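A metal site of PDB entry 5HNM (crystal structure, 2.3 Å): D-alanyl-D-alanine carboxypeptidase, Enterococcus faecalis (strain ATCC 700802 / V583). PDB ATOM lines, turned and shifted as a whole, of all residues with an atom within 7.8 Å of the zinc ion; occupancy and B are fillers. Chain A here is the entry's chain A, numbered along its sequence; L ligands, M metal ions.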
ATOM      1  N   SER A  72     -26.965 -21.026 -16.896  1.00  0.00           N
ATOM      2  CA  SER A  72     -26.959 -19.563 -16.980  1.00  0.00           C
ATOM      3  C   SER A  72     -26.033 -19.070 -18.082  1.00  0.00           C
ATOM      4  O   SER A  72     -24.879 -19.478 -18.156  1.00  0.00           O
ATOM      5  CB  SER A  72     -26.556 -18.958 -15.632  1.00  0.00           C
ATOM      6  OG  SER A  72     -26.511 -17.545 -15.707  1.00  0.00           O
ATOM      7  N   GLY A  73     -26.549 -18.180 -18.914  1.00  0.00           N
ATOM      8  CA  GLY A  73     -25.764 -17.578 -19.977  1.00  0.00           C
ATOM      9  C   GLY A  73     -25.681 -16.079 -19.798  1.00  0.00           C
ATOM     10  O   GLY A  73     -25.030 -15.586 -18.886  1.00  0.00           O
ATOM     11  N   ARG A  75     -26.753 -12.315 -18.787  1.00  0.00           N
ATOM     12  CA  ARG A  75     -27.466 -11.711 -17.668  1.00  0.00           C
ATOM     13  C   ARG A  75     -27.501 -10.199 -17.819  1.00  0.00           C
ATOM     14  O   ARG A  75     -26.481  -9.575 -18.117  1.00  0.00           O
ATOM     15  CB  ARG A  75     -26.819 -12.077 -16.332  1.00  0.00           C
ATOM     16  CG  ARG A  75     -26.765 -13.556 -16.019  1.00  0.00           C
ATOM     17  CD  ARG A  75     -26.054 -13.791 -14.705  1.00  0.00           C
ATOM     18  NE  ARG A  75     -25.651 -15.182 -14.536  1.00  0.00           N
ATOM     19  CZ  ARG A  75     -24.786 -15.607 -13.622  1.00  0.00           C
ATOM     20  NH1 ARG A  75     -24.223 -14.736 -12.793  1.00  0.00           N
ATOM     21  NH2 ARG A  75     -24.469 -16.889 -13.545  1.00  0.00           N
ATOM     22  N   GLN A  80     -27.687  -9.611 -12.509  1.00  0.00           N
ATOM     23  CA  GLN A  80     -26.478  -9.774 -11.706  1.00  0.00           C
ATOM     24  C   GLN A  80     -26.676  -9.140 -10.334  1.00  0.00           C
ATOM     25  O   GLN A  80     -26.199  -9.666  -9.329  1.00  0.00           O
ATOM     26  CB  GLN A  80     -25.272  -9.153 -12.400  1.00  0.00           C
ATOM     27  CG  GLN A  80     -24.467 -10.134 -13.238  1.00  0.00           C
ATOM     28  CD  GLN A  80     -23.675 -11.107 -12.394  1.00  0.00           C
ATOM     29  OE1 GLN A  80     -23.436 -12.249 -12.804  1.00  0.00           O
ATOM     30  NE2 GLN A  80     -23.253 -10.667 -11.218  1.00  0.00           N
ATOM     31  N   TRP A 108     -17.567 -14.808  -4.938  1.00  0.00           N
ATOM     32  CA  TRP A 108     -18.332 -15.788  -5.690  1.00  0.00           C
ATOM     33  C   TRP A 108     -19.083 -15.125  -6.844  1.00  0.00           C
ATOM     34  O   TRP A 108     -18.946 -15.519  -7.993  1.00  0.00           O
ATOM     35  CB  TRP A 108     -19.304 -16.532  -4.782  1.00  0.00           C
ATOM     36  CG  TRP A 108     -18.652 -17.455  -3.811  1.00  0.00           C
ATOM     37  CD1 TRP A 108     -18.391 -17.214  -2.489  1.00  0.00           C
ATOM     38  CD2 TRP A 108     -18.159 -18.780  -4.078  1.00  0.00           C
ATOM     39  NE1 TRP A 108     -17.773 -18.297  -1.916  1.00  0.00           N
ATOM     40  CE2 TRP A 108     -17.614 -19.275  -2.869  1.00  0.00           C
ATOM     41  CE3 TRP A 108     -18.119 -19.594  -5.214  1.00  0.00           C
ATOM     42  CZ2 TRP A 108     -17.051 -20.545  -2.769  1.00  0.00           C
ATOM     43  CZ3 TRP A 108     -17.563 -20.852  -5.117  1.00  0.00           C
ATOM     44  CH2 TRP A 108     -17.034 -21.320  -3.901  1.00  0.00           C
ATOM     45  N   SER A 115     -19.014  -8.808 -14.457  1.00  0.00           N
ATOM     46  CA  SER A 115     -19.336 -10.192 -14.783  1.00  0.00           C
ATOM     47  C   SER A 115     -19.264 -10.423 -16.284  1.00  0.00           C
ATOM     48  O   SER A 115     -19.812  -9.638 -17.065  1.00  0.00           O
ATOM     49  CB  SER A 115     -20.726 -10.554 -14.250  1.00  0.00           C
ATOM     50  OG  SER A 115     -21.089 -11.869 -14.633  1.00  0.00           O
ATOM     51  N   GLU A 116     -18.605 -11.496 -16.694  1.00  0.00           N
ATOM     52  CA  GLU A 116     -18.515 -11.817 -18.106  1.00  0.00           C
ATOM     53  C   GLU A 116     -19.781 -12.502 -18.601  1.00  0.00           C
ATOM     54  O   GLU A 116     -19.895 -12.858 -19.771  1.00  0.00           O
ATOM     55  CB  GLU A 116     -17.273 -12.676 -18.401  1.00  0.00           C
ATOM     56  CG  GLU A 116     -17.234 -14.008 -17.671  1.00  0.00           C
ATOM     57  CD  GLU A 116     -16.007 -14.825 -18.021  1.00  0.00           C
ATOM     58  OE1 GLU A 116     -15.023 -14.227 -18.507  1.00  0.00           O
ATOM     59  OE2 GLU A 116     -16.028 -16.050 -17.812  1.00  0.00           O
ATOM     60  N   HIS A 117     -20.739 -12.700 -17.687  1.00  0.00           N
ATOM     61  CA  HIS A 117     -22.063 -13.175 -18.069  1.00  0.00           C
ATOM     62  C   HIS A 117     -22.821 -12.074 -18.801  1.00  0.00           C
ATOM     63  O   HIS A 117     -23.790 -12.335 -19.508  1.00  0.00           O
ATOM     64  CB  HIS A 117     -22.857 -13.631 -16.837  1.00  0.00           C
ATOM     65  CG  HIS A 117     -22.514 -15.007 -16.386  1.00  0.00           C
ATOM     66  ND1 HIS A 117     -23.037 -16.144 -16.966  1.00  0.00           N
ATOM     67  CD2 HIS A 117     -21.684 -15.447 -15.399  1.00  0.00           C
ATOM     68  CE1 HIS A 117     -22.551 -17.216 -16.358  1.00  0.00           C
ATOM     69  NE2 HIS A 117     -21.732 -16.818 -15.407  1.00  0.00           N
ATOM     70  N   ALA A 122     -20.045 -16.254 -21.685  1.00  0.00           N
ATOM     71  CA  ALA A 122     -19.846 -17.160 -20.555  1.00  0.00           C
ATOM     72  C   ALA A 122     -21.111 -17.960 -20.272  1.00  0.00           C
ATOM     73  O   ALA A 122     -22.223 -17.428 -20.288  1.00  0.00           O
ATOM     74  CB  ALA A 122     -19.430 -16.378 -19.320  1.00  0.00           C
ATOM     75  N   VAL A 123     -20.944 -19.254 -20.004  1.00  0.00           N
ATOM     76  CA  VAL A 123     -22.067 -20.101 -19.672  1.00  0.00           C
ATOM     77  C   VAL A 123     -21.793 -20.910 -18.411  1.00  0.00           C
ATOM     78  O   VAL A 123     -20.695 -21.453 -18.233  1.00  0.00           O
ATOM     79  CB  VAL A 123     -22.411 -21.070 -20.827  1.00  0.00           C
ATOM     80  CG1 VAL A 123     -23.112 -20.331 -21.957  1.00  0.00           C
ATOM     81  CG2 VAL A 123     -21.156 -21.777 -21.339  1.00  0.00           C
ATOM     82  N   ASP A 124     -22.775 -20.961 -17.520  1.00  0.00           N
ATOM     83  CA  ASP A 124     -22.713 -21.847 -16.373  1.00  0.00           C
ATOM     84  C   ASP A 124     -23.284 -23.200 -16.769  1.00  0.00           C
ATOM     85  O   ASP A 124     -24.473 -23.318 -17.081  1.00  0.00           O
ATOM     86  CB  ASP A 124     -23.483 -21.261 -15.176  1.00  0.00           C
ATOM     87  CG  ASP A 124     -22.833 -20.005 -14.631  1.00  0.00           C
ATOM     88  OD1 ASP A 124     -21.595 -19.868 -14.778  1.00  0.00           O
ATOM     89  OD2 ASP A 124     -23.548 -19.173 -14.047  1.00  0.00           O
ATOM     90  N   ILE A 125     -22.440 -24.218 -16.778  1.00  0.00           N
ATOM     91  CA  ILE A 125     -22.835 -25.539 -17.236  1.00  0.00           C
ATOM     92  C   ILE A 125     -23.066 -26.493 -16.069  1.00  0.00           C
ATOM     93  O   ILE A 125     -22.216 -26.646 -15.197  1.00  0.00           O
ATOM     94  CB  ILE A 125     -21.778 -26.156 -18.176  1.00  0.00           C
ATOM     95  CG1 ILE A 125     -21.453 -25.183 -19.316  1.00  0.00           C
ATOM     96  CG2 ILE A 125     -22.269 -27.492 -18.729  1.00  0.00           C
ATOM     97  CD1 ILE A 125     -20.420 -25.697 -20.290  1.00  0.00           C
ATOM     98  N   ARG A 153     -12.952 -21.201 -16.664  1.00  0.00           N
ATOM     99  CA  ARG A 153     -12.560 -19.822 -16.432  1.00  0.00           C
ATOM    100  C   ARG A 153     -11.857 -19.571 -15.101  1.00  0.00           C
ATOM    101  O   ARG A 153     -10.930 -18.767 -15.035  1.00  0.00           O
ATOM    102  CB  ARG A 153     -13.798 -18.923 -16.525  1.00  0.00           C
ATOM    103  CG  ARG A 153     -13.501 -17.441 -16.422  1.00  0.00           C
ATOM    104  CD  ARG A 153     -12.523 -16.999 -17.485  1.00  0.00           C
ATOM    105  NE  ARG A 153     -12.231 -15.570 -17.406  1.00  0.00           N
ATOM    106  CZ  ARG A 153     -11.298 -15.054 -16.616  1.00  0.00           C
ATOM    107  NH1 ARG A 153     -10.558 -15.835 -15.844  1.00  0.00           N
ATOM    108  NH2 ARG A 153     -11.098 -13.732 -16.609  1.00  0.00           N
ATOM    109  N   TYR A 154     -12.302 -20.250 -14.042  1.00  0.00           N
ATOM    110  CA  TYR A 154     -11.757 -19.983 -12.724  1.00  0.00           C
ATOM    111  C   TYR A 154     -11.160 -21.229 -12.064  1.00  0.00           C
ATOM    112  O   TYR A 154     -11.841 -21.908 -11.294  1.00  0.00           O
ATOM    113  CB  TYR A 154     -12.840 -19.383 -11.820  1.00  0.00           C
ATOM    114  CG  TYR A 154     -13.534 -18.185 -12.428  1.00  0.00           C
ATOM    115  CD1 TYR A 154     -12.843 -16.990 -12.602  1.00  0.00           C
ATOM    116  CD2 TYR A 154     -14.861 -18.245 -12.819  1.00  0.00           C
ATOM    117  CE1 TYR A 154     -13.473 -15.883 -13.160  1.00  0.00           C
ATOM    118  CE2 TYR A 154     -15.488 -17.146 -13.382  1.00  0.00           C
ATOM    119  CZ  TYR A 154     -14.787 -15.967 -13.545  1.00  0.00           C
ATOM    120  OH  TYR A 154     -15.411 -14.873 -14.099  1.00  0.00           O
ATOM    121  N   GLU A 167     -14.965 -22.268  -9.356  1.00  0.00           N
ATOM    122  CA  GLU A 167     -16.258 -22.440 -10.024  1.00  0.00           C
ATOM    123  C   GLU A 167     -16.131 -23.352 -11.236  1.00  0.00           C
ATOM    124  O   GLU A 167     -15.994 -22.885 -12.366  1.00  0.00           O
ATOM    125  CB  GLU A 167     -16.831 -21.083 -10.437  1.00  0.00           C
ATOM    126  CG  GLU A 167     -17.149 -20.160  -9.277  1.00  0.00           C
ATOM    127  CD  GLU A 167     -17.828 -18.880  -9.720  1.00  0.00           C
ATOM    128  OE1 GLU A 167     -17.859 -18.607 -10.933  1.00  0.00           O
ATOM    129  OE2 GLU A 167     -18.334 -18.146  -8.843  1.00  0.00           O
ATOM    130  N   TRP A 169     -18.197 -24.865 -12.814  1.00  0.00           N
ATOM    131  CA  TRP A 169     -19.365 -24.798 -13.678  1.00  0.00           C
ATOM    132  C   TRP A 169     -19.278 -23.661 -14.685  1.00  0.00           C
ATOM    133  O   TRP A 169     -19.961 -23.669 -15.712  1.00  0.00           O
ATOM    134  CB  TRP A 169     -20.639 -24.659 -12.833  1.00  0.00           C
ATOM    135  CG  TRP A 169     -20.584 -23.507 -11.868  1.00  0.00           C
ATOM    136  CD1 TRP A 169     -20.777 -22.190 -12.151  1.00  0.00           C
ATOM    137  CD2 TRP A 169     -20.317 -23.581 -10.465  1.00  0.00           C
ATOM    138  NE1 TRP A 169     -20.645 -21.436 -11.006  1.00  0.00           N
ATOM    139  CE2 TRP A 169     -20.372 -22.273  -9.957  1.00  0.00           C
ATOM    140  CE3 TRP A 169     -20.041 -24.635  -9.584  1.00  0.00           C
ATOM    141  CZ2 TRP A 169     -20.162 -21.980  -8.616  1.00  0.00           C
ATOM    142  CZ3 TRP A 169     -19.831 -24.341  -8.243  1.00  0.00           C
ATOM    143  CH2 TRP A 169     -19.892 -23.023  -7.775  1.00  0.00           C
ATOM    144  N   HIS A 170     -18.438 -22.673 -14.393  1.00  0.00           N
ATOM    145  CA  HIS A 170     -18.318 -21.485 -15.233  1.00  0.00           C
ATOM    146  C   HIS A 170     -17.331 -21.698 -16.377  1.00  0.00           C
ATOM    147  O   HIS A 170     -16.144 -21.907 -16.150  1.00  0.00           O
ATOM    148  CB  HIS A 170     -17.902 -20.269 -14.405  1.00  0.00           C
ATOM    149  CG  HIS A 170     -17.950 -18.982 -15.155  1.00  0.00           C
ATOM    150  ND1 HIS A 170     -18.947 -18.053 -14.981  1.00  0.00           N
ATOM    151  CD2 HIS A 170     -17.126 -18.466 -16.098  1.00  0.00           C
ATOM    152  CE1 HIS A 170     -18.740 -17.020 -15.775  1.00  0.00           C
ATOM    153  NE2 HIS A 170     -17.631 -17.249 -16.465  1.00  0.00           N
ATOM    154  N   TYR A 171     -17.837 -21.642 -17.612  1.00  0.00           N
ATOM    155  CA  TYR A 171     -16.985 -21.779 -18.781  1.00  0.00           C
ATOM    156  C   TYR A 171     -17.126 -20.580 -19.709  1.00  0.00           C
ATOM    157  O   TYR A 171     -18.218 -20.048 -19.906  1.00  0.00           O
ATOM    158  CB  TYR A 171     -17.305 -23.081 -19.520  1.00  0.00           C
ATOM    159  CG  TYR A 171     -16.659 -24.293 -18.892  1.00  0.00           C
ATOM    160  CD1 TYR A 171     -17.233 -24.904 -17.782  1.00  0.00           C
ATOM    161  CD2 TYR A 171     -15.477 -24.810 -19.389  1.00  0.00           C
ATOM    162  CE1 TYR A 171     -16.635 -26.011 -17.191  1.00  0.00           C
ATOM    163  CE2 TYR A 171     -14.878 -25.920 -18.811  1.00  0.00           C
ATOM    164  CZ  TYR A 171     -15.464 -26.507 -17.709  1.00  0.00           C
ATOM    165  OH  TYR A 171     -14.864 -27.600 -17.135  1.00  0.00           O
HETATM  166  S1  LIG L   1     -22.211 -17.138 -11.026  1.00  0.00           S
HETATM  167  O1  LIG L   1     -22.606 -15.734 -11.052  1.00  0.00           O
HETATM  168  O2  LIG L   1     -21.841 -17.521  -9.671  1.00  0.00           O
HETATM  169  O3  LIG L   1     -23.324 -17.973 -11.470  1.00  0.00           O
HETATM  170  O4  LIG L   1     -21.065 -17.339 -11.922  1.00  0.00           O
HETATM  171 ZN    ZN M   1     -20.803 -18.145 -14.203  1.00  0.00          ZN
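The backbone carbonyl oxygen (O) of Ser 72 lies within hydrogen-bond range of the backbone NH (N) of Asp 124 (2.7 Å). The guanidinium group (NH1) of Arg 75 is in hydrogen-bond range of the side-chain amide oxygen (OE1) of Gln 80 (2.6 Å). The guanidinium group (NH2) of Arg 75 lies within salt-bridge range of the side-chain carboxylate (OD2) of Asp 124 (2.5 Å). The side-chain hydroxyl (OG) of Ser 72 lies within hydrogen-bond range of the guanidinium group (NE) of Arg 75 (2.8 Å). The backbone carbonyl oxygen (O) of Gly 73 lies within hydrogen-bond range of a ring nitrogen (ND1) of His 117. The backbone carbonyl oxygen (O) of His 117 is in hydrogen-bond range of the backbone NH (N) of Arg 75. The backbone carbonyl oxygen of His 170 lies within hydrogen-bond range of the backbone NH of Arg 153, 3.3 Å away. A ring nitrogen (NE2) of His 170 is in hydrogen-bond range of the side-chain carboxylate (OE2) of Glu 116 (2.4 Å).
Merely in contact with the zinc ion: Arg 75. Within 4 Å of the zinc ion: Arg 75, His 117, Asp 124 and His 170. The nearest printed residue that does not touch the zinc ion is Glu 167 (4.4 Å).
The zinc ion is bound by the side-chain carboxylate (OD1) of Asp 124 (2.0 Å), a ring nitrogen (ND1) of His 170 (2.0 Å), a ring nitrogen (NE2) of His 117 (2.0 Å) and an oxygen (O4) of the ligand (2.4 Å). The zinc ion has four donor atoms within binding distance.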
